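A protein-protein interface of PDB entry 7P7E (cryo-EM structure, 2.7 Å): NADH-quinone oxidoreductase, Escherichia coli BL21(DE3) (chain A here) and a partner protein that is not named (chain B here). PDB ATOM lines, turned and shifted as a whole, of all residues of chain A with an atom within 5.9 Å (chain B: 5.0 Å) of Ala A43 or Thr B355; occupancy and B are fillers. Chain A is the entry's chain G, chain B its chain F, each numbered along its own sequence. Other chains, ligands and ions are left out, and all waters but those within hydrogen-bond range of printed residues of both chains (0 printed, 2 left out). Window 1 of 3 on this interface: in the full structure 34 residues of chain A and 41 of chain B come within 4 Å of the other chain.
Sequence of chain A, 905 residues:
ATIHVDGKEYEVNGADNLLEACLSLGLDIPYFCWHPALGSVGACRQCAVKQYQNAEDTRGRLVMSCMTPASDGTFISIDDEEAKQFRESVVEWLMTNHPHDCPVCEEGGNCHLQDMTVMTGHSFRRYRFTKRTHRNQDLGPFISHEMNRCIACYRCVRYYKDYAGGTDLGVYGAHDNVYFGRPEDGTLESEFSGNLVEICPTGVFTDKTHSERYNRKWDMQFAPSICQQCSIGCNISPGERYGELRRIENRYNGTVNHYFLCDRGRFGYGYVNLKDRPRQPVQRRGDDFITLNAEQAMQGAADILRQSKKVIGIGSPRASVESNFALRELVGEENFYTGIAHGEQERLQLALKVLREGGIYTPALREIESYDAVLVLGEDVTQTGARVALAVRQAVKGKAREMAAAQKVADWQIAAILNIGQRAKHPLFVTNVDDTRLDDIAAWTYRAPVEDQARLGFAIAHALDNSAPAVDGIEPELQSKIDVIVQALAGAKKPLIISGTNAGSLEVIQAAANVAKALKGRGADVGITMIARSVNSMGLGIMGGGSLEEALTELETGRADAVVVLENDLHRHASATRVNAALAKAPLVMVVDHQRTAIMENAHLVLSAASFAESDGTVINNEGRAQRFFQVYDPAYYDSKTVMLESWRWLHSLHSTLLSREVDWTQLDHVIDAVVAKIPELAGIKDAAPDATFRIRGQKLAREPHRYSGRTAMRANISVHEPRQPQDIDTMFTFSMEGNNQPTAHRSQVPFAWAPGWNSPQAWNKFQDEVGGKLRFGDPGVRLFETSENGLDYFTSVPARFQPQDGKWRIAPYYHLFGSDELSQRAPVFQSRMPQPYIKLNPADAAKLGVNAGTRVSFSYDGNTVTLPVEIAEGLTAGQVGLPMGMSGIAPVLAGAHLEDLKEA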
ATOM      1  N   CYS A  33     -23.528  24.844   2.369  1.00  0.00           N
ATOM      2  CA  CYS A  33     -23.289  23.442   2.685  1.00  0.00           C
ATOM      3  C   CYS A  33     -23.394  23.132   4.173  1.00  0.00           C
ATOM      4  O   CYS A  33     -23.529  21.960   4.535  1.00  0.00           O
ATOM      5  CB  CYS A  33     -21.918  23.012   2.153  1.00  0.00           C
ATOM      6  SG  CYS A  33     -20.511  23.587   3.099  1.00  0.00           S
ATOM      7  N   VAL A  41     -18.616  20.948   6.713  1.00  0.00           N
ATOM      8  CA  VAL A  41     -17.723  20.215   5.821  1.00  0.00           C
ATOM      9  C   VAL A  41     -16.869  21.115   4.945  1.00  0.00           C
ATOM     10  O   VAL A  41     -15.851  20.651   4.407  1.00  0.00           O
ATOM     11  CB  VAL A  41     -18.519  19.223   4.946  1.00  0.00           C
ATOM     12  CG1 VAL A  41     -18.885  17.994   5.749  1.00  0.00           C
ATOM     13  CG2 VAL A  41     -19.756  19.889   4.364  1.00  0.00           C
ATOM     14  N   GLY A  42     -17.211  22.387   4.762  1.00  0.00           N
ATOM     15  CA  GLY A  42     -16.396  23.268   3.950  1.00  0.00           C
ATOM     16  C   GLY A  42     -16.494  23.047   2.457  1.00  0.00           C
ATOM     17  O   GLY A  42     -15.501  23.222   1.748  1.00  0.00           O
ATOM     18  N   ALA A  43     -17.669  22.669   1.953  1.00  0.00           N
ATOM     19  CA  ALA A  43     -17.809  22.394   0.528  1.00  0.00           C
ATOM     20  C   ALA A  43     -18.057  23.666  -0.277  1.00  0.00           C
ATOM     21  O   ALA A  43     -17.248  24.037  -1.127  1.00  0.00           O
ATOM     22  CB  ALA A  43     -18.933  21.382   0.295  1.00  0.00           C
ATOM     23  N   CYS A  44     -19.159  24.366  -0.003  1.00  0.00           N
ATOM     24  CA  CYS A  44     -19.638  25.410  -0.906  1.00  0.00           C
ATOM     25  C   CYS A  44     -18.757  26.657  -0.928  1.00  0.00           C
ATOM     26  O   CYS A  44     -18.864  27.446  -1.870  1.00  0.00           O
ATOM     27  CB  CYS A  44     -21.061  25.805  -0.528  1.00  0.00           C
ATOM     28  SG  CYS A  44     -21.167  26.683   1.027  1.00  0.00           S
ATOM     29  N   ARG A  45     -17.915  26.855   0.089  1.00  0.00           N
ATOM     30  CA  ARG A  45     -17.000  28.002   0.211  1.00  0.00           C
ATOM     31  C   ARG A  45     -17.731  29.345   0.218  1.00  0.00           C
ATOM     32  O   ARG A  45     -17.156  30.374  -0.137  1.00  0.00           O
ATOM     33  CB  ARG A  45     -15.909  27.991  -0.866  1.00  0.00           C
ATOM     34  CG  ARG A  45     -15.243  26.642  -1.080  1.00  0.00           C
ATOM     35  CD  ARG A  45     -14.686  26.048   0.194  1.00  0.00           C
ATOM     36  NE  ARG A  45     -13.350  26.531   0.504  1.00  0.00           N
ATOM     37  CZ  ARG A  45     -12.624  26.096   1.523  1.00  0.00           C
ATOM     38  NH1 ARG A  45     -13.072  25.155   2.336  1.00  0.00           N
ATOM     39  NH2 ARG A  45     -11.423  26.623   1.735  1.00  0.00           N
ATOM     40  N   GLN A  46     -18.989  29.357   0.651  1.00  0.00           N
ATOM     41  CA  GLN A  46     -19.785  30.576   0.661  1.00  0.00           C
ATOM     42  C   GLN A  46     -19.599  31.398   1.930  1.00  0.00           C
ATOM     43  O   GLN A  46     -19.748  32.622   1.888  1.00  0.00           O
ATOM     44  CB  GLN A  46     -21.267  30.225   0.480  1.00  0.00           C
ATOM     45  CG  GLN A  46     -22.211  31.401   0.314  1.00  0.00           C
ATOM     46  CD  GLN A  46     -21.982  32.152  -0.976  1.00  0.00           C
ATOM     47  OE1 GLN A  46     -22.379  31.698  -2.043  1.00  0.00           O
ATOM     48  NE2 GLN A  46     -21.335  33.303  -0.886  1.00  0.00           N
ATOM     49  N   CYS A  66     -17.545  28.341   8.854  1.00  0.00           N
ATOM     50  CA  CYS A  66     -18.092  27.079   9.337  1.00  0.00           C
ATOM     51  C   CYS A  66     -16.991  26.105   9.734  1.00  0.00           C
ATOM     52  O   CYS A  66     -17.202  25.258  10.606  1.00  0.00           O
ATOM     53  CB  CYS A  66     -19.013  26.460   8.283  1.00  0.00           C
ATOM     54  SG  CYS A  66     -18.186  25.740   6.856  1.00  0.00           S
ATOM     55  N   VAL A  90     -18.482  33.430  -5.419  1.00  0.00           N
ATOM     56  CA  VAL A  90     -19.006  32.083  -5.206  1.00  0.00           C
ATOM     57  C   VAL A  90     -20.451  31.997  -5.685  1.00  0.00           C
ATOM     58  O   VAL A  90     -20.844  31.034  -6.364  1.00  0.00           O
ATOM     59  CB  VAL A  90     -18.863  31.679  -3.725  1.00  0.00           C
ATOM     60  CG1 VAL A  90     -19.666  30.429  -3.419  1.00  0.00           C
ATOM     61  CG2 VAL A  90     -17.405  31.450  -3.383  1.00  0.00           C
ATOM     62  N   TRP A  93     -20.344  31.950  -9.503  1.00  0.00           N
ATOM     63  CA  TRP A  93     -19.945  30.633  -9.992  1.00  0.00           C
ATOM     64  C   TRP A  93     -21.099  29.646  -9.910  1.00  0.00           C
ATOM     65  O   TRP A  93     -21.279  28.817 -10.808  1.00  0.00           O
ATOM     66  CB  TRP A  93     -18.750  30.111  -9.198  1.00  0.00           C
ATOM     67  CG  TRP A  93     -17.461  30.799  -9.503  1.00  0.00           C
ATOM     68  CD1 TRP A  93     -17.039  31.244 -10.717  1.00  0.00           C
ATOM     69  CD2 TRP A  93     -16.421  31.116  -8.574  1.00  0.00           C
ATOM     70  NE1 TRP A  93     -15.802  31.823 -10.603  1.00  0.00           N
ATOM     71  CE2 TRP A  93     -15.400  31.757  -9.297  1.00  0.00           C
ATOM     72  CE3 TRP A  93     -16.255  30.921  -7.201  1.00  0.00           C
ATOM     73  CZ2 TRP A  93     -14.230  32.205  -8.692  1.00  0.00           C
ATOM     74  CZ3 TRP A  93     -15.097  31.370  -6.604  1.00  0.00           C
ATOM     75  CH2 TRP A  93     -14.098  32.001  -7.349  1.00  0.00           C
ATOM     76  N   LEU A  94     -21.892  29.721  -8.839  1.00  0.00           N
ATOM     77  CA  LEU A  94     -23.099  28.902  -8.777  1.00  0.00           C
ATOM     78  C   LEU A  94     -24.122  29.323  -9.827  1.00  0.00           C
ATOM     79  O   LEU A  94     -24.857  28.478 -10.346  1.00  0.00           O
ATOM     80  CB  LEU A  94     -23.711  28.966  -7.380  1.00  0.00           C
ATOM     81  CG  LEU A  94     -22.868  28.335  -6.274  1.00  0.00           C
ATOM     82  CD1 LEU A  94     -23.589  28.417  -4.949  1.00  0.00           C
ATOM     83  CD2 LEU A  94     -22.537  26.899  -6.620  1.00  0.00           C
ATOM     84  N   ILE A 151     -26.629  23.085  -6.869  1.00  0.00           N
ATOM     85  CA  ILE A 151     -25.419  23.865  -6.673  1.00  0.00           C
ATOM     86  C   ILE A 151     -24.306  23.024  -6.067  1.00  0.00           C
ATOM     87  O   ILE A 151     -23.264  23.567  -5.689  1.00  0.00           O
ATOM     88  CB  ILE A 151     -25.698  25.110  -5.820  1.00  0.00           C
ATOM     89  CG1 ILE A 151     -26.340  24.711  -4.493  1.00  0.00           C
ATOM     90  CG2 ILE A 151     -26.590  26.072  -6.575  1.00  0.00           C
ATOM     91  CD1 ILE A 151     -26.266  25.767  -3.440  1.00  0.00           C
ATOM     92  N   ALA A 152     -24.511  21.703  -5.972  1.00  0.00           N
ATOM     93  CA  ALA A 152     -23.532  20.735  -5.463  1.00  0.00           C
ATOM     94  C   ALA A 152     -23.045  21.105  -4.064  1.00  0.00           C
ATOM     95  O   ALA A 152     -21.847  21.202  -3.798  1.00  0.00           O
ATOM     96  CB  ALA A 152     -22.359  20.567  -6.430  1.00  0.00           C
ATOM     97  N   CYS A 153     -23.997  21.327  -3.166  1.00  0.00           N
ATOM     98  CA  CYS A 153     -23.679  21.694  -1.797  1.00  0.00           C
ATOM     99  C   CYS A 153     -23.602  20.496  -0.862  1.00  0.00           C
ATOM    100  O   CYS A 153     -23.246  20.671   0.308  1.00  0.00           O
ATOM    101  CB  CYS A 153     -24.711  22.694  -1.279  1.00  0.00           C
ATOM    102  SG  CYS A 153     -26.252  21.968  -0.727  1.00  0.00           S
ATOM    103  N   TYR A 154     -23.940  19.301  -1.344  1.00  0.00           N
ATOM    104  CA  TYR A 154     -23.812  18.017  -0.656  1.00  0.00           C
ATOM    105  C   TYR A 154     -24.677  17.906   0.595  1.00  0.00           C
ATOM    106  O   TYR A 154     -24.476  16.986   1.385  1.00  0.00           O
ATOM    107  CB  TYR A 154     -22.350  17.701  -0.299  1.00  0.00           C
ATOM    108  CG  TYR A 154     -21.458  17.486  -1.497  1.00  0.00           C
ATOM    109  CD1 TYR A 154     -20.888  18.561  -2.164  1.00  0.00           C
ATOM    110  CD2 TYR A 154     -21.185  16.209  -1.961  1.00  0.00           C
ATOM    111  CE1 TYR A 154     -20.077  18.369  -3.261  1.00  0.00           C
ATOM    112  CE2 TYR A 154     -20.374  16.007  -3.056  1.00  0.00           C
ATOM    113  CZ  TYR A 154     -19.824  17.091  -3.701  1.00  0.00           C
ATOM    114  OH  TYR A 154     -19.014  16.897  -4.793  1.00  0.00           O
ATOM    115  N   TRP B 353     -15.821  18.711  -5.186  1.00  0.00           N
ATOM    116  CA  TRP B 353     -16.246  18.971  -3.815  1.00  0.00           C
ATOM    117  C   TRP B 353     -16.583  20.441  -3.599  1.00  0.00           C
ATOM    118  O   TRP B 353     -17.619  20.767  -3.011  1.00  0.00           O
ATOM    119  CB  TRP B 353     -15.162  18.530  -2.835  1.00  0.00           C
ATOM    120  CG  TRP B 353     -15.490  18.783  -1.408  1.00  0.00           C
ATOM    121  CD1 TRP B 353     -14.887  19.677  -0.576  1.00  0.00           C
ATOM    122  CD2 TRP B 353     -16.496  18.128  -0.632  1.00  0.00           C
ATOM    123  NE1 TRP B 353     -15.457  19.622   0.669  1.00  0.00           N
ATOM    124  CE2 TRP B 353     -16.447  18.677   0.661  1.00  0.00           C
ATOM    125  CE3 TRP B 353     -17.434  17.130  -0.906  1.00  0.00           C
ATOM    126  CZ2 TRP B 353     -17.300  18.264   1.677  1.00  0.00           C
ATOM    127  CZ3 TRP B 353     -18.278  16.721   0.106  1.00  0.00           C
ATOM    128  CH2 TRP B 353     -18.207  17.287   1.379  1.00  0.00           C
ATOM    129  N   CYS B 354     -15.725  21.344  -4.059  1.00  0.00           N
ATOM    130  CA  CYS B 354     -15.832  22.731  -3.646  1.00  0.00           C
ATOM    131  C   CYS B 354     -16.034  23.663  -4.835  1.00  0.00           C
ATOM    132  O   CYS B 354     -15.538  23.420  -5.936  1.00  0.00           O
ATOM    133  CB  CYS B 354     -14.616  23.145  -2.795  1.00  0.00           C
ATOM    134  SG  CYS B 354     -13.094  23.561  -3.620  1.00  0.00           S
ATOM    135  N   THR B 355     -16.789  24.734  -4.570  1.00  0.00           N
ATOM    136  CA  THR B 355     -17.309  25.615  -5.617  1.00  0.00           C
ATOM    137  C   THR B 355     -16.259  26.296  -6.495  1.00  0.00           C
ATOM    138  O   THR B 355     -16.437  26.275  -7.724  1.00  0.00           O
ATOM    139  CB  THR B 355     -18.234  26.663  -4.984  1.00  0.00           C
ATOM    140  OG1 THR B 355     -19.221  26.014  -4.178  1.00  0.00           O
ATOM    141  CG2 THR B 355     -18.921  27.499  -6.050  1.00  0.00           C
ATOM    142  N   PRO B 356     -15.192  26.939  -5.971  1.00  0.00           N
ATOM    143  CA  PRO B 356     -14.329  27.729  -6.872  1.00  0.00           C
ATOM    144  C   PRO B 356     -13.636  26.906  -7.941  1.00  0.00           C
ATOM    145  O   PRO B 356     -13.696  27.269  -9.113  1.00  0.00           O
ATOM    146  CB  PRO B 356     -13.326  28.378  -5.909  1.00  0.00           C
ATOM    147  CG  PRO B 356     -13.999  28.372  -4.614  1.00  0.00           C
ATOM    148  CD  PRO B 356     -14.693  27.065  -4.590  1.00  0.00           C
ATOM    149  N   CYS B 357     -13.043  25.771  -7.576  1.00  0.00           N
ATOM    150  CA  CYS B 357     -12.423  24.898  -8.568  1.00  0.00           C
ATOM    151  C   CYS B 357     -13.457  24.348  -9.544  1.00  0.00           C
ATOM    152  O   CYS B 357     -13.361  24.590 -10.754  1.00  0.00           O
ATOM    153  CB  CYS B 357     -11.683  23.784  -7.832  1.00  0.00           C
ATOM    154  SG  CYS B 357     -11.089  22.322  -8.696  1.00  0.00           S
ATOM    155  N   ARG B 358     -14.525  23.740  -9.009  1.00  0.00           N
ATOM    156  CA  ARG B 358     -15.512  23.019  -9.812  1.00  0.00           C
ATOM    157  C   ARG B 358     -16.240  23.932 -10.793  1.00  0.00           C
ATOM    158  O   ARG B 358     -16.512  23.537 -11.932  1.00  0.00           O
ATOM    159  CB  ARG B 358     -16.515  22.322  -8.885  1.00  0.00           C
ATOM    160  CG  ARG B 358     -17.849  21.973  -9.530  1.00  0.00           C
ATOM    161  CD  ARG B 358     -18.843  21.372  -8.557  1.00  0.00           C
ATOM    162  NE  ARG B 358     -19.691  22.398  -7.966  1.00  0.00           N
ATOM    163  CZ  ARG B 358     -19.644  22.765  -6.695  1.00  0.00           C
ATOM    164  NH1 ARG B 358     -18.830  22.177  -5.836  1.00  0.00           N
ATOM    165  NH2 ARG B 358     -20.440  23.741  -6.273  1.00  0.00           N
ATOM    166  N   ASP B 359     -16.562  25.155 -10.377  1.00  0.00           N
ATOM    167  CA  ASP B 359     -17.348  26.065 -11.197  1.00  0.00           C
ATOM    168  C   ASP B 359     -16.553  27.262 -11.704  1.00  0.00           C
ATOM    169  O   ASP B 359     -17.139  28.157 -12.320  1.00  0.00           O
ATOM    170  CB  ASP B 359     -18.572  26.548 -10.417  1.00  0.00           C
ATOM    171  CG  ASP B 359     -19.617  25.466 -10.249  1.00  0.00           C
ATOM    172  OD1 ASP B 359     -19.764  24.629 -11.163  1.00  0.00           O
ATOM    173  OD2 ASP B 359     -20.297  25.451  -9.204  1.00  0.00           O
ATOM    174  N   GLY B 360     -15.243  27.303 -11.487  1.00  0.00           N
ATOM    175  CA  GLY B 360     -14.466  28.411 -11.986  1.00  0.00           C
ATOM    176  C   GLY B 360     -13.377  27.972 -12.932  1.00  0.00           C
ATOM    177  O   GLY B 360     -12.959  28.758 -13.784  1.00  0.00           O
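The backbone carbonyl oxygen of Ile A151 sits at hydrogen-bond distance from the guanidinium group of Arg B358, 2.9 Å away.
O of Cys A44 is in hydrogen-bond range of OG1 of Thr B355.
The side-chain sulfur (SG) of Cys A33 sits close to the backbone NH (N) of Ala A43 (3.2 Å).
SG of Cys A44 sits close to N of Gln A46 (3.5 Å).
The side-chain hydroxyl of Thr B355 is in hydrogen-bond range of the guanidinium group of Arg B358 (3.3 Å).
The side-chain carboxylate (OD2) of Asp B359 lies within salt-bridge range of the guanidinium group (NE) of Arg B358 (3.3 Å).
The backbone carbonyl oxygen of Trp B353 lies within hydrogen-bond range of the guanidinium group of Arg B358 (3.4 Å).
The backbone carbonyl oxygen of Gly A42 sits at hydrogen-bond distance from the guanidinium group of Arg A45, at 3.2 Å.
Among the printed residues, merely in contact across the chains: Ala A43 with Cys B354, Tyr A154 with Trp B353, Trp A93 with Asp B359, Ala A152 with Arg B358, Ala A43 with Thr B355, Trp A93 with Pro B356, Arg A45 with Pro B356, Ala A43 with Trp B353, Val A41 with Trp B353, Leu A94 with Thr B355, Leu A94 with Asp B359, Gly A42 with Trp B353, Leu A94 with Arg B358, Trp A93 with Gly B360 and Arg A45 with Cys B354.
Ala A43 touches just these residues of chain B: Trp B353 (3.6 Å), Cys B354 (3.2 Å) and Thr B355 (3.5 Å).
Of the printed residues of chain A, Thr B355 touches Ala A43 (3.5 Å), Cys A44 (2.7 Å) and Leu A94 (3.7 Å).
Of the printed residues of chain B, Leu A94 touches Thr B355, Arg B358 and Asp B359.
Of the printed residues of chain A, Asp B359 touches Trp A93 and Leu A94.
Of the printed residues of chain B, Gly A42 touches Trp B353.
Of the printed residues of chain B, Tyr A154 touches Trp B353 (3.4 Å).
Printed residues of chain A within 4 Å of Trp B353: Val A41, Gly A42, Ala A43 and Tyr A154.
Cys A33 touches none of the printed residues of chain B.
Gln A46 touches none of the printed residues of chain B.
The nearest printed residue of chain B that does not touch Ala A43 is Pro B356 (5.3 Å).
The nearest printed residue of chain A that does not touch Thr B355 is Val A90 (4.01 Å).
The nearest printed residue of chain B that does not touch Val A41 is Cys B354 (7.7 Å).
Of the 8 printed residues of chain B, 7 touch a printed residue of chain A.
Printed residues of chain B that touch a printed residue of chain A: Trp B353, Cys B354, Thr B355, Pro B356, Arg B358, Asp B359 and Gly B360.
Hydrophobic or aromatic side chains of chain B within 4 Å of the printed part of chain A: Trp B353 and Pro B356.
Printed residues of chain A that touch a printed residue of chain B: Val A41, Gly A42, Ala A43, Cys A44, Arg A45, Trp A93, Leu A94, Ile A151, Ala A152 and Tyr A154.
Hydrophobic or aromatic side chains of chain A that line the printed part of chain B: Val A41, Ala A43, Trp A93, Leu A94, Ala A152 and Tyr A154.
Among the printed residues, 17 pairs touch across the chains.
Among the printed residues, no Asp or Glu carboxylate lies within 4 Å of a Lys or Arg side-chain nitrogen of the other chain.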
